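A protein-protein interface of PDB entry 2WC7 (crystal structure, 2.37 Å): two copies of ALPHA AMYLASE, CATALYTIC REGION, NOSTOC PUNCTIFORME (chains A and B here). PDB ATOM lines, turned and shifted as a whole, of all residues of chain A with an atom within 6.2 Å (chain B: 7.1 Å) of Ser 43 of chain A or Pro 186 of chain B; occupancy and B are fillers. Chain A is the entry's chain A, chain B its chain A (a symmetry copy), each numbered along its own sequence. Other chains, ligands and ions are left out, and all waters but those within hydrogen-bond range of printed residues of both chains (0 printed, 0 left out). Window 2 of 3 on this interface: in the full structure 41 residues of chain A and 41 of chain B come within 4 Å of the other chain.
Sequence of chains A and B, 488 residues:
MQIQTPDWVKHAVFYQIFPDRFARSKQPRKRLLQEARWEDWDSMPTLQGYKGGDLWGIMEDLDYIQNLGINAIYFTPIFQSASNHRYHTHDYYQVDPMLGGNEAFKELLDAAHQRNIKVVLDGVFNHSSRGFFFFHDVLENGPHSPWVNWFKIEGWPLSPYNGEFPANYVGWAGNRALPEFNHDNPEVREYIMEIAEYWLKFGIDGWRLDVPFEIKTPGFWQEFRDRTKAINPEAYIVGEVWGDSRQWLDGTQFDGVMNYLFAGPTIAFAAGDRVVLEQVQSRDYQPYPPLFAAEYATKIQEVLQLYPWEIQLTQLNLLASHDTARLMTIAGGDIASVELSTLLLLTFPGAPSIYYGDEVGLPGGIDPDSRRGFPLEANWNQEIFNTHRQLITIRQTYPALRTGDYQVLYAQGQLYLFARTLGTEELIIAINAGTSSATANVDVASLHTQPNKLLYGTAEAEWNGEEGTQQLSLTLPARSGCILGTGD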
ATOM      1  N   LEU A  33      12.731   8.551  10.871  1.00  0.00           N
ATOM      2  CA  LEU A  33      11.324   8.644  10.493  1.00  0.00           C
ATOM      3  C   LEU A  33      10.978  10.086  10.123  1.00  0.00           C
ATOM      4  O   LEU A  33      10.363  10.799  10.911  1.00  0.00           O
ATOM      5  CB  LEU A  33      10.447   8.176  11.664  1.00  0.00           C
ATOM      6  CG  LEU A  33      10.210   6.680  11.960  1.00  0.00           C
ATOM      7  CD1 LEU A  33      11.137   5.785  11.148  1.00  0.00           C
ATOM      8  CD2 LEU A  33      10.376   6.442  13.461  1.00  0.00           C
ATOM      9  N   GLU A  39       2.892  15.324  16.920  1.00  0.00           N
ATOM     10  CA  GLU A  39       2.016  14.830  17.977  1.00  0.00           C
ATOM     11  C   GLU A  39       2.517  13.495  18.525  1.00  0.00           C
ATOM     12  O   GLU A  39       2.260  13.149  19.676  1.00  0.00           O
ATOM     13  CB  GLU A  39       0.589  14.644  17.448  1.00  0.00           C
ATOM     14  CG  GLU A  39      -0.022  15.872  16.780  1.00  0.00           C
ATOM     15  CD  GLU A  39       0.670  16.246  15.475  1.00  0.00           C
ATOM     16  OE1 GLU A  39       0.854  15.348  14.623  1.00  0.00           O
ATOM     17  OE2 GLU A  39       1.021  17.435  15.297  1.00  0.00           O
ATOM     18  N   ASP A  40       3.234  12.752  17.690  1.00  0.00           N
ATOM     19  CA  ASP A  40       3.763  11.445  18.071  1.00  0.00           C
ATOM     20  C   ASP A  40       5.157  11.508  18.684  1.00  0.00           C
ATOM     21  O   ASP A  40       5.626  10.528  19.266  1.00  0.00           O
ATOM     22  CB  ASP A  40       3.802  10.516  16.849  1.00  0.00           C
ATOM     23  CG  ASP A  40       2.423  10.217  16.290  1.00  0.00           C
ATOM     24  OD1 ASP A  40       1.581   9.676  17.041  1.00  0.00           O
ATOM     25  OD2 ASP A  40       2.182  10.517  15.098  1.00  0.00           O
ATOM     26  N   TRP A  41       5.816  12.655  18.543  1.00  0.00           N
ATOM     27  CA  TRP A  41       7.166  12.845  19.065  1.00  0.00           C
ATOM     28  C   TRP A  41       7.408  12.131  20.395  1.00  0.00           C
ATOM     29  O   TRP A  41       8.348  11.347  20.515  1.00  0.00           O
ATOM     30  CB  TRP A  41       7.463  14.342  19.206  1.00  0.00           C
ATOM     31  CG  TRP A  41       8.861  14.658  19.661  1.00  0.00           C
ATOM     32  CD1 TRP A  41       9.268  14.941  20.937  1.00  0.00           C
ATOM     33  CD2 TRP A  41      10.037  14.720  18.842  1.00  0.00           C
ATOM     34  NE1 TRP A  41      10.625  15.176  20.961  1.00  0.00           N
ATOM     35  CE2 TRP A  41      11.121  15.046  19.690  1.00  0.00           C
ATOM     36  CE3 TRP A  41      10.279  14.529  17.475  1.00  0.00           C
ATOM     37  CZ2 TRP A  41      12.428  15.187  19.214  1.00  0.00           C
ATOM     38  CZ3 TRP A  41      11.576  14.668  17.002  1.00  0.00           C
ATOM     39  CH2 TRP A  41      12.635  14.996  17.872  1.00  0.00           C
ATOM     40  N   ASP A  42       6.558  12.386  21.384  1.00  0.00           N
ATOM     41  CA  ASP A  42       6.712  11.762  22.698  1.00  0.00           C
ATOM     42  C   ASP A  42       6.522  10.246  22.688  1.00  0.00           C
ATOM     43  O   ASP A  42       7.053   9.545  23.551  1.00  0.00           O
ATOM     44  CB  ASP A  42       5.747  12.400  23.696  1.00  0.00           C
ATOM     45  CG  ASP A  42       6.069  13.860  23.965  1.00  0.00           C
ATOM     46  OD1 ASP A  42       5.342  14.489  24.763  1.00  0.00           O
ATOM     47  OD2 ASP A  42       7.047  14.379  23.380  1.00  0.00           O
ATOM     48  N   SER A  43       5.766   9.744  21.717  1.00  0.00           N
ATOM     49  CA  SER A  43       5.528   8.307  21.596  1.00  0.00           C
ATOM     50  C   SER A  43       6.756   7.612  21.030  1.00  0.00           C
ATOM     51  O   SER A  43       6.895   6.396  21.142  1.00  0.00           O
ATOM     52  CB  SER A  43       4.347   8.030  20.665  1.00  0.00           C
ATOM     53  OG  SER A  43       3.136   8.515  21.209  1.00  0.00           O
ATOM     54  N   MET A  44       7.642   8.397  20.424  1.00  0.00           N
ATOM     55  CA  MET A  44       8.851   7.863  19.806  1.00  0.00           C
ATOM     56  C   MET A  44      10.115   8.142  20.625  1.00  0.00           C
ATOM     57  O   MET A  44      10.829   9.116  20.382  1.00  0.00           O
ATOM     58  CB  MET A  44       8.975   8.433  18.389  1.00  0.00           C
ATOM     59  CG  MET A  44       7.661   8.357  17.623  1.00  0.00           C
ATOM     60  SD  MET A  44       7.748   8.749  15.865  1.00  0.00           S
ATOM     61  CE  MET A  44       6.769   7.451  15.183  1.00  0.00           C
ATOM     62  N   PRO A  45      10.406   7.265  21.604  1.00  0.00           N
ATOM     63  CA  PRO A  45      11.556   7.329  22.513  1.00  0.00           C
ATOM     64  C   PRO A  45      12.911   7.575  21.848  1.00  0.00           C
ATOM     65  O   PRO A  45      13.712   8.366  22.349  1.00  0.00           O
ATOM     66  CB  PRO A  45      11.508   5.974  23.217  1.00  0.00           C
ATOM     67  CG  PRO A  45      10.051   5.687  23.273  1.00  0.00           C
ATOM     68  CD  PRO A  45       9.598   6.065  21.889  1.00  0.00           C
ATOM     69  N   GLN A  48      12.644  11.238  20.204  1.00  0.00           N
ATOM     70  CA  GLN A  48      12.332  12.282  21.172  1.00  0.00           C
ATOM     71  C   GLN A  48      13.520  12.559  22.088  1.00  0.00           C
ATOM     72  O   GLN A  48      13.747  13.696  22.502  1.00  0.00           O
ATOM     73  CB  GLN A  48      11.108  11.894  22.004  1.00  0.00           C
ATOM     74  CG  GLN A  48      10.884  12.771  23.225  1.00  0.00           C
ATOM     75  CD  GLN A  48      11.729  12.345  24.410  1.00  0.00           C
ATOM     76  OE1 GLN A  48      11.894  11.154  24.674  1.00  0.00           O
ATOM     77  NE2 GLN A  48      12.269  13.320  25.132  1.00  0.00           N
ATOM     78  N   ASN B 149      13.399  -2.294  21.380  1.00  0.00           N
ATOM     79  CA  ASN B 149      11.946  -2.260  21.481  1.00  0.00           C
ATOM     80  C   ASN B 149      11.273  -2.285  20.112  1.00  0.00           C
ATOM     81  O   ASN B 149      10.046  -2.252  20.012  1.00  0.00           O
ATOM     82  CB  ASN B 149      11.492  -1.027  22.267  1.00  0.00           C
ATOM     83  CG  ASN B 149       9.993  -0.997  22.487  1.00  0.00           C
ATOM     84  OD1 ASN B 149       9.408  -1.953  22.998  1.00  0.00           O
ATOM     85  ND2 ASN B 149       9.360   0.105  22.102  1.00  0.00           N
ATOM     86  N   TRP B 150      12.084  -2.344  19.060  1.00  0.00           N
ATOM     87  CA  TRP B 150      11.569  -2.474  17.703  1.00  0.00           C
ATOM     88  C   TRP B 150      11.165  -3.913  17.401  1.00  0.00           C
ATOM     89  O   TRP B 150      10.463  -4.180  16.426  1.00  0.00           O
ATOM     90  CB  TRP B 150      12.608  -1.994  16.688  1.00  0.00           C
ATOM     91  CG  TRP B 150      12.498  -0.538  16.359  1.00  0.00           C
ATOM     92  CD1 TRP B 150      12.311   0.489  17.237  1.00  0.00           C
ATOM     93  CD2 TRP B 150      12.570   0.056  15.056  1.00  0.00           C
ATOM     94  NE1 TRP B 150      12.260   1.685  16.564  1.00  0.00           N
ATOM     95  CE2 TRP B 150      12.418   1.447  15.222  1.00  0.00           C
ATOM     96  CE3 TRP B 150      12.747  -0.453  13.766  1.00  0.00           C
ATOM     97  CZ2 TRP B 150      12.437   2.334  14.149  1.00  0.00           C
ATOM     98  CZ3 TRP B 150      12.767   0.431  12.702  1.00  0.00           C
ATOM     99  CH2 TRP B 150      12.613   1.808  12.899  1.00  0.00           C
ATOM    100  N   ASN B 182       7.879  -5.268  16.398  1.00  0.00           N
ATOM    101  CA  ASN B 182       6.966  -4.900  17.472  1.00  0.00           C
ATOM    102  C   ASN B 182       6.125  -3.762  16.888  1.00  0.00           C
ATOM    103  O   ASN B 182       6.422  -2.583  17.087  1.00  0.00           O
ATOM    104  CB  ASN B 182       7.749  -4.422  18.688  1.00  0.00           C
ATOM    105  CG  ASN B 182       6.857  -3.919  19.803  1.00  0.00           C
ATOM    106  OD1 ASN B 182       5.634  -4.045  19.748  1.00  0.00           O
ATOM    107  ND2 ASN B 182       7.470  -3.343  20.828  1.00  0.00           N
ATOM    108  N   HIS B 183       5.088  -4.129  16.142  1.00  0.00           N
ATOM    109  CA  HIS B 183       4.212  -3.162  15.500  1.00  0.00           C
ATOM    110  C   HIS B 183       3.508  -2.234  16.470  1.00  0.00           C
ATOM    111  O   HIS B 183       3.065  -1.151  16.083  1.00  0.00           O
ATOM    112  CB  HIS B 183       3.174  -3.887  14.641  1.00  0.00           C
ATOM    113  CG  HIS B 183       3.765  -4.932  13.749  1.00  0.00           C
ATOM    114  ND1 HIS B 183       4.001  -6.223  14.174  1.00  0.00           N
ATOM    115  CD2 HIS B 183       4.216  -4.864  12.476  1.00  0.00           C
ATOM    116  CE1 HIS B 183       4.570  -6.904  13.196  1.00  0.00           C
ATOM    117  NE2 HIS B 183       4.713  -6.103  12.154  1.00  0.00           N
ATOM    118  N   ASP B 184       3.392  -2.661  17.724  1.00  0.00           N
ATOM    119  CA  ASP B 184       2.751  -1.836  18.736  1.00  0.00           C
ATOM    120  C   ASP B 184       3.585  -0.587  18.942  1.00  0.00           C
ATOM    121  O   ASP B 184       3.086   0.429  19.419  1.00  0.00           O
ATOM    122  CB  ASP B 184       2.632  -2.595  20.059  1.00  0.00           C
ATOM    123  CG  ASP B 184       1.450  -3.543  20.081  1.00  0.00           C
ATOM    124  OD1 ASP B 184       1.276  -4.246  21.098  1.00  0.00           O
ATOM    125  OD2 ASP B 184       0.694  -3.579  19.087  1.00  0.00           O
ATOM    126  N   ASN B 185       4.861  -0.674  18.580  1.00  0.00           N
ATOM    127  CA  ASN B 185       5.780   0.448  18.710  1.00  0.00           C
ATOM    128  C   ASN B 185       5.469   1.456  17.598  1.00  0.00           C
ATOM    129  O   ASN B 185       5.614   1.141  16.418  1.00  0.00           O
ATOM    130  CB  ASN B 185       7.212  -0.052  18.569  1.00  0.00           C
ATOM    131  CG  ASN B 185       8.239   1.002  18.926  1.00  0.00           C
ATOM    132  OD1 ASN B 185       8.014   2.198  18.740  1.00  0.00           O
ATOM    133  ND2 ASN B 185       9.386   0.558  19.422  1.00  0.00           N
ATOM    134  N   PRO B 186       5.045   2.681  17.958  1.00  0.00           N
ATOM    135  CA  PRO B 186       4.719   3.697  16.950  1.00  0.00           C
ATOM    136  C   PRO B 186       5.850   4.016  15.975  1.00  0.00           C
ATOM    137  O   PRO B 186       5.608   4.539  14.880  1.00  0.00           O
ATOM    138  CB  PRO B 186       4.290   4.903  17.791  1.00  0.00           C
ATOM    139  CG  PRO B 186       5.051   4.720  19.053  1.00  0.00           C
ATOM    140  CD  PRO B 186       4.940   3.241  19.317  1.00  0.00           C
ATOM    141  N   GLU B 187       7.078   3.690  16.370  1.00  0.00           N
ATOM    142  CA  GLU B 187       8.239   3.924  15.516  1.00  0.00           C
ATOM    143  C   GLU B 187       8.268   2.878  14.400  1.00  0.00           C
ATOM    144  O   GLU B 187       8.389   3.218  13.227  1.00  0.00           O
ATOM    145  CB  GLU B 187       9.536   3.866  16.338  1.00  0.00           C
ATOM    146  CG  GLU B 187       9.538   4.805  17.549  1.00  0.00           C
ATOM    147  CD  GLU B 187      10.927   5.040  18.129  1.00  0.00           C
ATOM    148  OE1 GLU B 187      11.737   4.083  18.188  1.00  0.00           O
ATOM    149  OE2 GLU B 187      11.199   6.189  18.537  1.00  0.00           O
ATOM    150  N   VAL B 188       8.156   1.608  14.775  1.00  0.00           N
ATOM    151  CA  VAL B 188       8.137   0.511  13.815  1.00  0.00           C
ATOM    152  C   VAL B 188       7.052   0.776  12.778  1.00  0.00           C
ATOM    153  O   VAL B 188       7.255   0.605  11.574  1.00  0.00           O
ATOM    154  CB  VAL B 188       7.810  -0.822  14.519  1.00  0.00           C
ATOM    155  CG1 VAL B 188       7.634  -1.933  13.488  1.00  0.00           C
ATOM    156  CG2 VAL B 188       8.911  -1.164  15.522  1.00  0.00           C
ATOM    157  N   ARG B 189       5.897   1.198  13.267  1.00  0.00           N
ATOM    158  CA  ARG B 189       4.744   1.490  12.433  1.00  0.00           C
ATOM    159  C   ARG B 189       5.051   2.610  11.453  1.00  0.00           C
ATOM    160  O   ARG B 189       4.782   2.493  10.259  1.00  0.00           O
ATOM    161  CB  ARG B 189       3.579   1.864  13.335  1.00  0.00           C
ATOM    162  CG  ARG B 189       2.357   2.414  12.667  1.00  0.00           C
ATOM    163  CD  ARG B 189       1.225   2.308  13.671  1.00  0.00           C
ATOM    164  NE  ARG B 189       0.039   3.050  13.278  1.00  0.00           N
ATOM    165  CZ  ARG B 189      -1.149   2.886  13.845  1.00  0.00           C
ATOM    166  NH1 ARG B 189      -1.304   2.001  14.824  1.00  0.00           N
ATOM    167  NH2 ARG B 189      -2.181   3.614  13.438  1.00  0.00           N
ATOM    168  N   GLU B 190       5.615   3.697  11.959  1.00  0.00           N
ATOM    169  CA  GLU B 190       5.967   4.811  11.103  1.00  0.00           C
ATOM    170  C   GLU B 190       6.945   4.340  10.018  1.00  0.00           C
ATOM    171  O   GLU B 190       6.875   4.771   8.867  1.00  0.00           O
ATOM    172  CB  GLU B 190       6.613   5.923  11.932  1.00  0.00           C
ATOM    173  CG  GLU B 190       7.032   7.123  11.102  1.00  0.00           C
ATOM    174  CD  GLU B 190       5.866   7.687  10.322  1.00  0.00           C
ATOM    175  OE1 GLU B 190       4.727   7.544  10.812  1.00  0.00           O
ATOM    176  OE2 GLU B 190       6.084   8.270   9.236  1.00  0.00           O
ATOM    177  N   TYR B 191       7.857   3.453  10.398  1.00  0.00           N
ATOM    178  CA  TYR B 191       8.842   2.926   9.464  1.00  0.00           C
ATOM    179  C   TYR B 191       8.154   2.124   8.360  1.00  0.00           C
ATOM    180  O   TYR B 191       8.487   2.279   7.184  1.00  0.00           O
ATOM    181  CB  TYR B 191       9.864   2.051  10.208  1.00  0.00           C
ATOM    182  CG  TYR B 191      11.041   1.595   9.364  1.00  0.00           C
ATOM    183  CD1 TYR B 191      11.102   0.293   8.854  1.00  0.00           C
ATOM    184  CD2 TYR B 191      12.097   2.466   9.069  1.00  0.00           C
ATOM    185  CE1 TYR B 191      12.185  -0.133   8.071  1.00  0.00           C
ATOM    186  CE2 TYR B 191      13.185   2.047   8.285  1.00  0.00           C
ATOM    187  CZ  TYR B 191      13.220   0.747   7.790  1.00  0.00           C
ATOM    188  OH  TYR B 191      14.280   0.321   7.016  1.00  0.00           O
ATOM    189  N   GLU B 223      -4.542   3.131   8.837  1.00  0.00           N
ATOM    190  CA  GLU B 223      -3.540   4.151   8.575  1.00  0.00           C
ATOM    191  C   GLU B 223      -2.825   3.781   7.283  1.00  0.00           C
ATOM    192  O   GLU B 223      -2.568   4.639   6.439  1.00  0.00           O
ATOM    193  CB  GLU B 223      -2.525   4.245   9.720  1.00  0.00           C
ATOM    194  CG  GLU B 223      -1.380   5.205   9.425  1.00  0.00           C
ATOM    195  CD  GLU B 223      -0.502   5.495  10.629  1.00  0.00           C
ATOM    196  OE1 GLU B 223       0.568   6.113  10.445  1.00  0.00           O
ATOM    197  OE2 GLU B 223      -0.875   5.118  11.760  1.00  0.00           O
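NE1 of Trp 150 of chain B is in hydrogen-bond range of OE1 of Glu 187 of chain B, at 2.9 Å.
N of Glu 187 of chain B sits at hydrogen-bond distance from OD1 of Asn 185 of chain B, at 3.0 Å.
OE2 of Glu 187 of chain B sits close to O of Met 44 of chain A (3.5 Å).
OE2 of Glu 187 of chain B lies close to N of Pro 45 of chain A.
No position is printed for both chains.
Of the 7 pairs that touch across the chains among the printed residues, none has its exchanged pair printed and touching as well.
O of Glu 187 of chain B touches CD2 of Leu 33 of chain A (3.8 Å).
Glu 190 of chain B touches Leu 33 of chain A.
O of Ser 43 of chain A touches CG of Pro 186 of chain B, 3.3 Å away.
Pro 186 of chain B touches Met 44 of chain A (O to CE, 3.1 Å).
CE of Met 44 of chain A touches CB of Glu 190 of chain B, 3.6 Å away.
Printed residues of chain B that touch a printed residue of chain A: Pro 186, Glu 187 and Glu 190.
Hydrophobic or aromatic side chains of chain B within 4 Å of the printed part of chain A: Pro 186.
Printed residues of chain A that touch a printed residue of chain B: Leu 33, Ser 43, Met 44 and Pro 45.
Hydrophobic or aromatic side chains of chain A that line the printed part of chain B: Leu 33, Met 44 and Pro 45.
Ser 43 of chain A touches just one residue of chain B: Pro 186.
Pro 186 of chain B touches just these residues of chain A: Ser 43 and Met 44.
Printed residues of chain B within 4 Å of Leu 33 of chain A: Glu 187 and Glu 190.
Of the printed residues of chain B, Pro 45 of chain A touches Glu 187.
Printed residues of chain B within 4 Å of Met 44 of chain A: Pro 186, Glu 187 and Glu 190.
Printed residues of chain A within 4 Å of Glu 187 of chain B: Leu 33, Met 44 and Pro 45.
Of the printed residues of chain A, Glu 190 of chain B touches Leu 33 and Met 44.
Asp 42 of chain A touches none of the printed residues of chain B.
The nearest printed residue of chain A that does not touch Glu 187 of chain B is Ser 43 of chain A (4.7 Å).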
